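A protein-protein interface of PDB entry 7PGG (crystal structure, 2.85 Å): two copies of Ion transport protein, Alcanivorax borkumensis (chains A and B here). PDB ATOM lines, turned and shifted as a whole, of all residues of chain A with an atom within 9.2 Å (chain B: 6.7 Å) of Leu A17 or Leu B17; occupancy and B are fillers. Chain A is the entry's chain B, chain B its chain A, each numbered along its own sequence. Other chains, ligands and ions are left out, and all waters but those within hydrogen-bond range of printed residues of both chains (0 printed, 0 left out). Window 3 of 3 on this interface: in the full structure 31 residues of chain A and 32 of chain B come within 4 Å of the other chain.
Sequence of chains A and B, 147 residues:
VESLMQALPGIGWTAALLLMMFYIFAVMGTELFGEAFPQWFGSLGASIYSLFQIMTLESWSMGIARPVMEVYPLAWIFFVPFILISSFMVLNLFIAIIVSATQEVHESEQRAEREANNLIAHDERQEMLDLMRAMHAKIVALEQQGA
Of the 24 printed residues of chain A, 5 touch a printed residue of chain B.
Hydrophobic or aromatic side chains of chain A within 4 Å of the printed part of chain B: Trp A13, Ala A16, Leu A17 and Leu A19.
Of the 12 printed residues of chain B, 5 touch a printed residue of chain A.
Printed residues of chain B that touch a printed residue of chain A: Trp B13, Thr B14, Leu B17, Met B21 and Met B89.
Hydrophobic or aromatic side chains of chain B within 4 Å of the printed part of chain A: Trp B13, Leu B17, Met B21 and Met B89.
Among the printed residues, 8 pairs touch across the chains.
CA of Gly A12 touches CE of Met B89, 3.5 Å away.
Trp B13 touches Trp A13.
Trp A13 touches Leu B17.
CB of Ala A16 touches CD1 of Leu B17, at 3.6 Å.
Met B21 touches Ala A16.
Leu B17 touches Leu A17 (CD2 to CD2, 3.7 Å).
CD1 of Leu A19 touches CE of Met B21 (3.4 Å).
Gly A12 touches Met B89, but with the chains exchanged Met A89 does not touch Gly B12 (15.6 Å).
Trp B13 touches its own counterpart, Trp A13.
Ala A16 touches Leu B17, but with the chains exchanged Leu A17 does not touch Ala B16 (8.2 Å).
Leu A17 touches its own counterpart, Leu B17.
Positions printed for both chains: 12, 13, 14, 15, 16, 17, 18, 19, 20, 21, 22 and 89.
Leu B17 touches just these residues of chain A: Trp A13, Ala A16 and Leu A17.
No residue of chain A comes within 4 Å of Ala B16.
Printed residues of chain B within 4 Å of Gly A12: Met B89 (3.5 Å).
Of the printed residues of chain A, Trp B13 touches Trp A13 (3.2 Å).
Printed residues of chain B within 4 Å of Trp A13: Trp B13 (3.2 Å), Thr B14 (2.9 Å) and Leu B17 (3.8 Å).
Printed residues of chain A within 4 Å of Met B21: Ala A16 (3.4 Å) and Leu A19 (3.4 Å).
Of the printed residues of chain A, Met B89 touches Gly A12 (3.5 Å).
The nearest residue of chain A that does not touch Leu B17 is Gly A12 (4.7 Å).
The nearest printed residue of chain A that does not touch Thr B14 is Pro A9 (4.5 Å).
The backbone carbonyl oxygen (O) of Pro A9 lies close to the indole nitrogen (NE1) of Trp A13, at 3.3 Å.
The side-chain hydroxyl of Thr B14 is in hydrogen-bond range of the indole nitrogen of Trp A13, 2.9 Å away.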
ATOM      1  N   PRO A   9      17.038  -6.719 -12.993  1.00  0.00           N
ATOM      2  CA  PRO A   9      18.023  -6.421 -11.937  1.00  0.00           C
ATOM      3  C   PRO A   9      17.675  -5.192 -11.118  1.00  0.00           C
ATOM      4  O   PRO A   9      17.940  -5.164  -9.910  1.00  0.00           O
ATOM      5  CB  PRO A   9      19.331  -6.242 -12.719  1.00  0.00           C
ATOM      6  CG  PRO A   9      19.132  -7.031 -13.953  1.00  0.00           C
ATOM      7  CD  PRO A   9      17.689  -6.871 -14.307  1.00  0.00           C
ATOM      8  N   GLY A  10      17.077  -4.176 -11.739  1.00  0.00           N
ATOM      9  CA  GLY A  10      16.628  -3.025 -10.980  1.00  0.00           C
ATOM     10  C   GLY A  10      15.406  -3.303 -10.133  1.00  0.00           C
ATOM     11  O   GLY A  10      15.238  -2.698  -9.072  1.00  0.00           O
ATOM     12  N   ILE A  11      14.535  -4.202 -10.594  1.00  0.00           N
ATOM     13  CA  ILE A  11      13.397  -4.646  -9.789  1.00  0.00           C
ATOM     14  C   ILE A  11      13.889  -5.288  -8.495  1.00  0.00           C
ATOM     15  O   ILE A  11      13.364  -5.024  -7.407  1.00  0.00           O
ATOM     16  CB  ILE A  11      12.551  -5.648 -10.592  1.00  0.00           C
ATOM     17  CG1 ILE A  11      11.998  -5.107 -11.925  1.00  0.00           C
ATOM     18  CG2 ILE A  11      11.384  -6.139  -9.734  1.00  0.00           C
ATOM     19  CD1 ILE A  11      10.717  -4.451 -11.972  1.00  0.00           C
ATOM     20  N   GLY A  12      14.895  -6.162  -8.600  1.00  0.00           N
ATOM     21  CA  GLY A  12      15.419  -6.813  -7.413  1.00  0.00           C
ATOM     22  C   GLY A  12      16.076  -5.844  -6.455  1.00  0.00           C
ATOM     23  O   GLY A  12      15.999  -6.018  -5.237  1.00  0.00           O
ATOM     24  N   TRP A  13      16.728  -4.811  -6.989  1.00  0.00           N
ATOM     25  CA  TRP A  13      17.316  -3.778  -6.145  1.00  0.00           C
ATOM     26  C   TRP A  13      16.244  -3.090  -5.310  1.00  0.00           C
ATOM     27  O   TRP A  13      16.431  -2.856  -4.110  1.00  0.00           O
ATOM     28  CB  TRP A  13      18.050  -2.768  -7.025  1.00  0.00           C
ATOM     29  CG  TRP A  13      19.210  -3.374  -7.736  1.00  0.00           C
ATOM     30  CD1 TRP A  13      19.812  -4.565  -7.455  1.00  0.00           C
ATOM     31  CD2 TRP A  13      19.831  -2.884  -8.929  1.00  0.00           C
ATOM     32  NE1 TRP A  13      20.813  -4.816  -8.358  1.00  0.00           N
ATOM     33  CE2 TRP A  13      20.841  -3.802  -9.279  1.00  0.00           C
ATOM     34  CE3 TRP A  13      19.651  -1.746  -9.720  1.00  0.00           C
ATOM     35  CZ2 TRP A  13      21.664  -3.617 -10.386  1.00  0.00           C
ATOM     36  CZ3 TRP A  13      20.468  -1.564 -10.819  1.00  0.00           C
ATOM     37  CH2 TRP A  13      21.460  -2.497 -11.145  1.00  0.00           C
ATOM     38  N   THR A  14      15.110  -2.764  -5.933  1.00  0.00           N
ATOM     39  CA  THR A  14      13.987  -2.195  -5.196  1.00  0.00           C
ATOM     40  C   THR A  14      13.393  -3.211  -4.227  1.00  0.00           C
ATOM     41  O   THR A  14      13.131  -2.893  -3.062  1.00  0.00           O
ATOM     42  CB  THR A  14      12.921  -1.700  -6.173  1.00  0.00           C
ATOM     43  OG1 THR A  14      13.472  -0.675  -7.010  1.00  0.00           O
ATOM     44  CG2 THR A  14      11.715  -1.157  -5.427  1.00  0.00           C
ATOM     45  N   ALA A  15      13.171  -4.440  -4.697  1.00  0.00           N
ATOM     46  CA  ALA A  15      12.613  -5.474  -3.833  1.00  0.00           C
ATOM     47  C   ALA A  15      13.557  -5.794  -2.681  1.00  0.00           C
ATOM     48  O   ALA A  15      13.112  -6.040  -1.553  1.00  0.00           O
ATOM     49  CB  ALA A  15      12.311  -6.731  -4.646  1.00  0.00           C
ATOM     50  N   ALA A  16      14.864  -5.798  -2.945  1.00  0.00           N
ATOM     51  CA  ALA A  16      15.825  -6.068  -1.881  1.00  0.00           C
ATOM     52  C   ALA A  16      15.774  -4.984  -0.814  1.00  0.00           C
ATOM     53  O   ALA A  16      15.606  -5.275   0.376  1.00  0.00           O
ATOM     54  CB  ALA A  16      17.236  -6.191  -2.451  1.00  0.00           C
ATOM     55  N   LEU A  17      15.907  -3.722  -1.224  1.00  0.00           N
ATOM     56  CA  LEU A  17      15.888  -2.623  -0.269  1.00  0.00           C
ATOM     57  C   LEU A  17      14.536  -2.485   0.418  1.00  0.00           C
ATOM     58  O   LEU A  17      14.459  -1.876   1.487  1.00  0.00           O
ATOM     59  CB  LEU A  17      16.272  -1.320  -0.972  1.00  0.00           C
ATOM     60  CG  LEU A  17      17.702  -1.312  -1.521  1.00  0.00           C
ATOM     61  CD1 LEU A  17      17.990  -0.043  -2.312  1.00  0.00           C
ATOM     62  CD2 LEU A  17      18.716  -1.498  -0.405  1.00  0.00           C
ATOM     63  N   LEU A  18      13.475  -3.045  -0.165  1.00  0.00           N
ATOM     64  CA  LEU A  18      12.172  -3.023   0.492  1.00  0.00           C
ATOM     65  C   LEU A  18      12.159  -3.923   1.721  1.00  0.00           C
ATOM     66  O   LEU A  18      11.727  -3.507   2.803  1.00  0.00           O
ATOM     67  CB  LEU A  18      11.076  -3.440  -0.487  1.00  0.00           C
ATOM     68  CG  LEU A  18       9.656  -3.424   0.086  1.00  0.00           C
ATOM     69  CD1 LEU A  18       9.260  -2.021   0.525  1.00  0.00           C
ATOM     70  CD2 LEU A  18       8.656  -3.975  -0.923  1.00  0.00           C
ATOM     71  N   LEU A  19      12.613  -5.172   1.572  1.00  0.00           N
ATOM     72  CA  LEU A  19      12.716  -6.048   2.733  1.00  0.00           C
ATOM     73  C   LEU A  19      13.739  -5.522   3.729  1.00  0.00           C
ATOM     74  O   LEU A  19      13.622  -5.779   4.934  1.00  0.00           O
ATOM     75  CB  LEU A  19      13.060  -7.473   2.300  1.00  0.00           C
ATOM     76  CG  LEU A  19      11.953  -8.177   1.509  1.00  0.00           C
ATOM     77  CD1 LEU A  19      12.395  -9.542   1.018  1.00  0.00           C
ATOM     78  CD2 LEU A  19      10.694  -8.296   2.352  1.00  0.00           C
ATOM     79  N   MET A  20      14.740  -4.783   3.250  1.00  0.00           N
ATOM     80  CA  MET A  20      15.683  -4.093   4.127  1.00  0.00           C
ATOM     81  C   MET A  20      14.984  -3.052   4.985  1.00  0.00           C
ATOM     82  O   MET A  20      15.297  -2.899   6.167  1.00  0.00           O
ATOM     83  CB  MET A  20      16.799  -3.424   3.321  1.00  0.00           C
ATOM     84  CG  MET A  20      17.752  -4.387   2.664  1.00  0.00           C
ATOM     85  SD  MET A  20      18.529  -5.531   4.028  1.00  0.00           S
ATOM     86  CE  MET A  20      19.527  -4.215   5.052  1.00  0.00           C
ATOM     87  N   MET A  21      14.046  -2.332   4.379  1.00  0.00           N
ATOM     88  CA  MET A  21      13.284  -1.325   5.101  1.00  0.00           C
ATOM     89  C   MET A  21      12.451  -1.934   6.227  1.00  0.00           C
ATOM     90  O   MET A  21      12.331  -1.339   7.295  1.00  0.00           O
ATOM     91  CB  MET A  21      12.394  -0.521   4.145  1.00  0.00           C
ATOM     92  CG  MET A  21      13.171   0.413   3.216  1.00  0.00           C
ATOM     93  SD  MET A  21      14.176   1.552   4.434  1.00  0.00           S
ATOM     94  CE  MET A  21      14.936   2.863   3.308  1.00  0.00           C
ATOM     95  N   PHE A  22      11.886  -3.122   6.001  1.00  0.00           N
ATOM     96  CA  PHE A  22      11.137  -3.776   7.069  1.00  0.00           C
ATOM     97  C   PHE A  22      12.044  -4.125   8.241  1.00  0.00           C
ATOM     98  O   PHE A  22      11.755  -3.768   9.390  1.00  0.00           O
ATOM     99  CB  PHE A  22      10.423  -5.018   6.538  1.00  0.00           C
ATOM    100  CG  PHE A  22       9.179  -4.721   5.754  1.00  0.00           C
ATOM    101  CD1 PHE A  22       8.619  -3.458   5.772  1.00  0.00           C
ATOM    102  CD2 PHE A  22       8.530  -5.730   5.053  1.00  0.00           C
ATOM    103  CE1 PHE A  22       7.458  -3.190   5.069  1.00  0.00           C
ATOM    104  CE2 PHE A  22       7.367  -5.471   4.350  1.00  0.00           C
ATOM    105  CZ  PHE A  22       6.830  -4.200   4.357  1.00  0.00           C
ATOM    106  N   TYR A  23      13.169  -4.787   7.960  1.00  0.00           N
ATOM    107  CA  TYR A  23      14.076  -5.218   9.021  1.00  0.00           C
ATOM    108  C   TYR A  23      14.596  -4.054   9.858  1.00  0.00           C
ATOM    109  O   TYR A  23      14.660  -4.158  11.087  1.00  0.00           O
ATOM    110  CB  TYR A  23      15.233  -6.024   8.424  1.00  0.00           C
ATOM    111  CG  TYR A  23      16.392  -6.271   9.374  1.00  0.00           C
ATOM    112  CD1 TYR A  23      16.274  -7.130  10.475  1.00  0.00           C
ATOM    113  CD2 TYR A  23      17.637  -5.681   9.120  1.00  0.00           C
ATOM    114  CE1 TYR A  23      17.359  -7.351  11.320  1.00  0.00           C
ATOM    115  CE2 TYR A  23      18.719  -5.905   9.949  1.00  0.00           C
ATOM    116  CZ  TYR A  23      18.570  -6.736  11.041  1.00  0.00           C
ATOM    117  OH  TYR A  23      19.655  -6.949  11.865  1.00  0.00           O
ATOM    118  N   ILE A  24      14.979  -2.942   9.228  1.00  0.00           N
ATOM    119  CA  ILE A  24      15.539  -1.843  10.015  1.00  0.00           C
ATOM    120  C   ILE A  24      14.457  -1.176  10.859  1.00  0.00           C
ATOM    121  O   ILE A  24      14.699  -0.799  12.011  1.00  0.00           O
ATOM    122  CB  ILE A  24      16.274  -0.837   9.110  1.00  0.00           C
ATOM    123  CG1 ILE A  24      15.322  -0.173   8.110  1.00  0.00           C
ATOM    124  CG2 ILE A  24      17.420  -1.538   8.406  1.00  0.00           C
ATOM    125  CD1 ILE A  24      15.945   1.016   7.410  1.00  0.00           C
ATOM    126  N   PHE A  25      13.247  -1.028  10.313  1.00  0.00           N
ATOM    127  CA  PHE A  25      12.141  -0.521  11.116  1.00  0.00           C
ATOM    128  C   PHE A  25      11.601  -1.567  12.081  1.00  0.00           C
ATOM    129  O   PHE A  25      11.016  -1.206  13.108  1.00  0.00           O
ATOM    130  CB  PHE A  25      11.018   0.006  10.220  1.00  0.00           C
ATOM    131  CG  PHE A  25      11.324   1.329   9.569  1.00  0.00           C
ATOM    132  CD1 PHE A  25      11.126   2.510  10.262  1.00  0.00           C
ATOM    133  CD2 PHE A  25      11.804   1.395   8.272  1.00  0.00           C
ATOM    134  CE1 PHE A  25      11.402   3.730   9.679  1.00  0.00           C
ATOM    135  CE2 PHE A  25      12.084   2.612   7.682  1.00  0.00           C
ATOM    136  CZ  PHE A  25      11.883   3.781   8.387  1.00  0.00           C
ATOM    137  N   PHE A  82       8.293   5.302   7.670  1.00  0.00           N
ATOM    138  CA  PHE A  82       8.065   3.918   7.269  1.00  0.00           C
ATOM    139  C   PHE A  82       7.037   3.823   6.149  1.00  0.00           C
ATOM    140  O   PHE A  82       7.306   3.243   5.090  1.00  0.00           O
ATOM    141  CB  PHE A  82       7.622   3.082   8.467  1.00  0.00           C
ATOM    142  CG  PHE A  82       7.266   1.670   8.108  1.00  0.00           C
ATOM    143  CD1 PHE A  82       8.250   0.745   7.808  1.00  0.00           C
ATOM    144  CD2 PHE A  82       5.939   1.272   8.061  1.00  0.00           C
ATOM    145  CE1 PHE A  82       7.917  -0.550   7.470  1.00  0.00           C
ATOM    146  CE2 PHE A  82       5.602  -0.020   7.726  1.00  0.00           C
ATOM    147  CZ  PHE A  82       6.590  -0.932   7.429  1.00  0.00           C
ATOM    148  N   ILE A  85       8.452   5.504   2.812  1.00  0.00           N
ATOM    149  CA  ILE A  85       9.543   4.863   2.084  1.00  0.00           C
ATOM    150  C   ILE A  85       9.117   3.497   1.555  1.00  0.00           C
ATOM    151  O   ILE A  85       9.554   3.081   0.475  1.00  0.00           O
ATOM    152  CB  ILE A  85      10.804   4.770   2.965  1.00  0.00           C
ATOM    153  CG1 ILE A  85      12.021   4.420   2.108  1.00  0.00           C
ATOM    154  CG2 ILE A  85      10.639   3.738   4.069  1.00  0.00           C
ATOM    155  CD1 ILE A  85      12.403   5.499   1.116  1.00  0.00           C
ATOM    156  N   SER A  86       8.240   2.793   2.278  1.00  0.00           N
ATOM    157  CA  SER A  86       7.827   1.460   1.850  1.00  0.00           C
ATOM    158  C   SER A  86       6.853   1.557   0.686  1.00  0.00           C
ATOM    159  O   SER A  86       6.835   0.690  -0.193  1.00  0.00           O
ATOM    160  CB  SER A  86       7.078   0.733   2.957  1.00  0.00           C
ATOM    161  OG  SER A  86       7.564   0.938   4.245  1.00  0.00           O
ATOM    162  N   MET A  89       8.773   2.449  -2.500  1.00  0.00           N
ATOM    163  CA  MET A  89       9.447   1.317  -3.112  1.00  0.00           C
ATOM    164  C   MET A  89       8.473   0.467  -3.923  1.00  0.00           C
ATOM    165  O   MET A  89       8.778   0.065  -5.047  1.00  0.00           O
ATOM    166  CB  MET A  89      10.126   0.409  -2.094  1.00  0.00           C
ATOM    167  CG  MET A  89      11.296   0.915  -1.266  1.00  0.00           C
ATOM    168  SD  MET A  89      12.721   2.057  -1.925  1.00  0.00           S
ATOM    169  CE  MET A  89      13.019   1.621  -3.763  1.00  0.00           C
ATOM    170  N   VAL A  90       7.311   0.175  -3.332  1.00  0.00           N
ATOM    171  CA  VAL A  90       6.281  -0.578  -4.045  1.00  0.00           C
ATOM    172  C   VAL A  90       5.863   0.167  -5.306  1.00  0.00           C
ATOM    173  O   VAL A  90       5.600  -0.444  -6.349  1.00  0.00           O
ATOM    174  CB  VAL A  90       5.080  -0.850  -3.119  1.00  0.00           C
ATOM    175  CG1 VAL A  90       3.956  -1.530  -3.887  1.00  0.00           C
ATOM    176  CG2 VAL A  90       5.507  -1.701  -1.937  1.00  0.00           C
ATOM    177  N   ASN A  92       7.873   2.086  -7.083  1.00  0.00           N
ATOM    178  CA  ASN A  92       8.961   1.920  -8.041  1.00  0.00           C
ATOM    179  C   ASN A  92       8.989   0.529  -8.659  1.00  0.00           C
ATOM    180  O   ASN A  92       9.579   0.356  -9.730  1.00  0.00           O
ATOM    181  CB  ASN A  92      10.301   2.224  -7.374  1.00  0.00           C
ATOM    182  CG  ASN A  92      10.465   3.693  -7.040  1.00  0.00           C
ATOM    183  OD1 ASN A  92      10.097   4.565  -7.823  1.00  0.00           O
ATOM    184  ND2 ASN A  92      11.028   3.974  -5.869  1.00  0.00           N
ATOM    185  N   LEU A  93       8.381  -0.465  -8.009  1.00  0.00           N
ATOM    186  CA  LEU A  93       8.257  -1.780  -8.632  1.00  0.00           C
ATOM    187  C   LEU A  93       7.364  -1.720  -9.864  1.00  0.00           C
ATOM    188  O   LEU A  93       7.674  -2.329 -10.895  1.00  0.00           O
ATOM    189  CB  LEU A  93       7.715  -2.797  -7.627  1.00  0.00           C
ATOM    190  CG  LEU A  93       8.627  -3.176  -6.460  1.00  0.00           C
ATOM    191  CD1 LEU A  93       7.889  -4.064  -5.471  1.00  0.00           C
ATOM    192  CD2 LEU A  93       9.874  -3.876  -6.977  1.00  0.00           C
ATOM    193  N   GLY B  12      27.648  -6.020  -8.815  1.00  0.00           N
ATOM    194  CA  GLY B  12      27.954  -5.892  -7.401  1.00  0.00           C
ATOM    195  C   GLY B  12      26.751  -5.482  -6.575  1.00  0.00           C
ATOM    196  O   GLY B  12      26.591  -5.924  -5.438  1.00  0.00           O
ATOM    197  N   TRP B  13      25.894  -4.629  -7.138  1.00  0.00           N
ATOM    198  CA  TRP B  13      24.671  -4.227  -6.448  1.00  0.00           C
ATOM    199  C   TRP B  13      23.785  -5.434  -6.167  1.00  0.00           C
ATOM    200  O   TRP B  13      23.246  -5.579  -5.063  1.00  0.00           O
ATOM    201  CB  TRP B  13      23.936  -3.199  -7.303  1.00  0.00           C
ATOM    202  CG  TRP B  13      24.712  -1.934  -7.464  1.00  0.00           C
ATOM    203  CD1 TRP B  13      25.790  -1.534  -6.728  1.00  0.00           C
ATOM    204  CD2 TRP B  13      24.552  -0.959  -8.499  1.00  0.00           C
ATOM    205  NE1 TRP B  13      26.268  -0.336  -7.201  1.00  0.00           N
ATOM    206  CE2 TRP B  13      25.528   0.034  -8.292  1.00  0.00           C
ATOM    207  CE3 TRP B  13      23.658  -0.815  -9.563  1.00  0.00           C
ATOM    208  CZ2 TRP B  13      25.635   1.155  -9.112  1.00  0.00           C
ATOM    209  CZ3 TRP B  13      23.765   0.293 -10.374  1.00  0.00           C
ATOM    210  CH2 TRP B  13      24.747   1.266 -10.147  1.00  0.00           C
ATOM    211  N   THR B  14      23.632  -6.315  -7.158  1.00  0.00           N
ATOM    212  CA  THR B  14      22.886  -7.551  -6.950  1.00  0.00           C
ATOM    213  C   THR B  14      23.615  -8.472  -5.979  1.00  0.00           C
ATOM    214  O   THR B  14      23.007  -9.019  -5.051  1.00  0.00           O
ATOM    215  CB  THR B  14      22.660  -8.257  -8.288  1.00  0.00           C
ATOM    216  OG1 THR B  14      21.899  -7.409  -9.156  1.00  0.00           O
ATOM    217  CG2 THR B  14      21.919  -9.564  -8.081  1.00  0.00           C
ATOM    218  N   ALA B  15      24.920  -8.663  -6.184  1.00  0.00           N
ATOM    219  CA  ALA B  15      25.694  -9.515  -5.286  1.00  0.00           C
ATOM    220  C   ALA B  15      25.701  -8.957  -3.870  1.00  0.00           C
ATOM    221  O   ALA B  15      25.649  -9.717  -2.895  1.00  0.00           O
ATOM    222  CB  ALA B  15      27.121  -9.672  -5.807  1.00  0.00           C
ATOM    223  N   ALA B  16      25.766  -7.631  -3.738  1.00  0.00           N
ATOM    224  CA  ALA B  16      25.746  -7.027  -2.412  1.00  0.00           C
ATOM    225  C   ALA B  16      24.430  -7.305  -1.704  1.00  0.00           C
ATOM    226  O   ALA B  16      24.410  -7.836  -0.587  1.00  0.00           O
ATOM    227  CB  ALA B  16      26.005  -5.522  -2.492  1.00  0.00           C
ATOM    228  N   LEU B  17      23.316  -6.954  -2.344  1.00  0.00           N
ATOM    229  CA  LEU B  17      22.010  -7.161  -1.738  1.00  0.00           C
ATOM    230  C   LEU B  17      21.698  -8.638  -1.536  1.00  0.00           C
ATOM    231  O   LEU B  17      20.834  -8.971  -0.720  1.00  0.00           O
ATOM    232  CB  LEU B  17      20.938  -6.494  -2.599  1.00  0.00           C
ATOM    233  CG  LEU B  17      21.083  -4.972  -2.682  1.00  0.00           C
ATOM    234  CD1 LEU B  17      20.080  -4.366  -3.653  1.00  0.00           C
ATOM    235  CD2 LEU B  17      20.956  -4.341  -1.307  1.00  0.00           C
ATOM    236  N   LEU B  18      22.389  -9.532  -2.247  1.00  0.00           N
ATOM    237  CA  LEU B  18      22.196 -10.962  -2.028  1.00  0.00           C
ATOM    238  C   LEU B  18      22.747 -11.394  -0.675  1.00  0.00           C
ATOM    239  O   LEU B  18      22.065 -12.086   0.090  1.00  0.00           O
ATOM    240  CB  LEU B  18      22.848 -11.764  -3.153  1.00  0.00           C
ATOM    241  CG  LEU B  18      22.684 -13.283  -3.046  1.00  0.00           C
ATOM    242  CD1 LEU B  18      21.216 -13.678  -3.105  1.00  0.00           C
ATOM    243  CD2 LEU B  18      23.475 -13.996  -4.133  1.00  0.00           C
ATOM    244  N   LEU B  19      23.990 -11.013  -0.366  1.00  0.00           N
ATOM    245  CA  LEU B  19      24.540 -11.327   0.949  1.00  0.00           C
ATOM    246  C   LEU B  19      23.778 -10.613   2.055  1.00  0.00           C
ATOM    247  O   LEU B  19      23.717 -11.108   3.186  1.00  0.00           O
ATOM    248  CB  LEU B  19      26.025 -10.977   1.011  1.00  0.00           C
ATOM    249  CG  LEU B  19      26.905 -11.857   0.125  1.00  0.00           C
ATOM    250  CD1 LEU B  19      28.346 -11.382   0.145  1.00  0.00           C
ATOM    251  CD2 LEU B  19      26.804 -13.310   0.563  1.00  0.00           C
ATOM    252  N   MET B  20      23.199  -9.458   1.753  1.00  0.00           N
ATOM    253  CA  MET B  20      22.370  -8.786   2.748  1.00  0.00           C
ATOM    254  C   MET B  20      21.062  -9.530   2.959  1.00  0.00           C
ATOM    255  O   MET B  20      20.496  -9.478   4.051  1.00  0.00           O
ATOM    256  CB  MET B  20      22.092  -7.337   2.355  1.00  0.00           C
ATOM    257  CG  MET B  20      22.729  -6.325   3.293  1.00  0.00           C
ATOM    258  SD  MET B  20      22.910  -4.582   2.462  1.00  0.00           S
ATOM    259  CE  MET B  20      23.970  -5.130   0.931  1.00  0.00           C
ATOM    260  N   MET B  21      20.601 -10.246   1.938  1.00  0.00           N
ATOM    261  CA  MET B  21      19.404 -11.068   2.050  1.00  0.00           C
ATOM    262  C   MET B  21      19.637 -12.240   3.011  1.00  0.00           C
ATOM    263  O   MET B  21      18.747 -12.630   3.766  1.00  0.00           O
ATOM    264  CB  MET B  21      18.974 -11.563   0.666  1.00  0.00           C
ATOM    265  CG  MET B  21      17.623 -11.020   0.247  1.00  0.00           C
ATOM    266  SD  MET B  21      17.333  -9.248   1.007  1.00  0.00           S
ATOM    267  CE  MET B  21      15.646  -8.834   0.168  1.00  0.00           C
ATOM    268  N   PHE B  22      20.850 -12.795   2.986  1.00  0.00           N
ATOM    269  CA  PHE B  22      21.185 -13.868   3.917  1.00  0.00           C
ATOM    270  C   PHE B  22      21.219 -13.361   5.355  1.00  0.00           C
ATOM    271  O   PHE B  22      20.578 -13.939   6.243  1.00  0.00           O
ATOM    272  CB  PHE B  22      22.520 -14.503   3.532  1.00  0.00           C
ATOM    273  CG  PHE B  22      22.439 -15.447   2.368  1.00  0.00           C
ATOM    274  CD1 PHE B  22      21.216 -15.891   1.902  1.00  0.00           C
ATOM    275  CD2 PHE B  22      23.597 -15.945   1.782  1.00  0.00           C
ATOM    276  CE1 PHE B  22      21.143 -16.784   0.845  1.00  0.00           C
ATOM    277  CE2 PHE B  22      23.534 -16.841   0.725  1.00  0.00           C
ATOM    278  CZ  PHE B  22      22.307 -17.261   0.257  1.00  0.00           C
ATOM    279  N   MET B  89      17.719 -12.922  -7.187  1.00  0.00           N
ATOM    280  CA  MET B  89      18.994 -12.197  -7.217  1.00  0.00           C
ATOM    281  C   MET B  89      20.015 -12.964  -8.043  1.00  0.00           C
ATOM    282  O   MET B  89      20.686 -12.394  -8.902  1.00  0.00           O
ATOM    283  CB  MET B  89      19.474 -11.977  -5.775  1.00  0.00           C
ATOM    284  CG  MET B  89      18.479 -11.079  -5.074  1.00  0.00           C
ATOM    285  SD  MET B  89      18.617  -9.160  -5.171  1.00  0.00           S
ATOM    286  CE  MET B  89      18.332  -8.700  -7.008  1.00  0.00           C
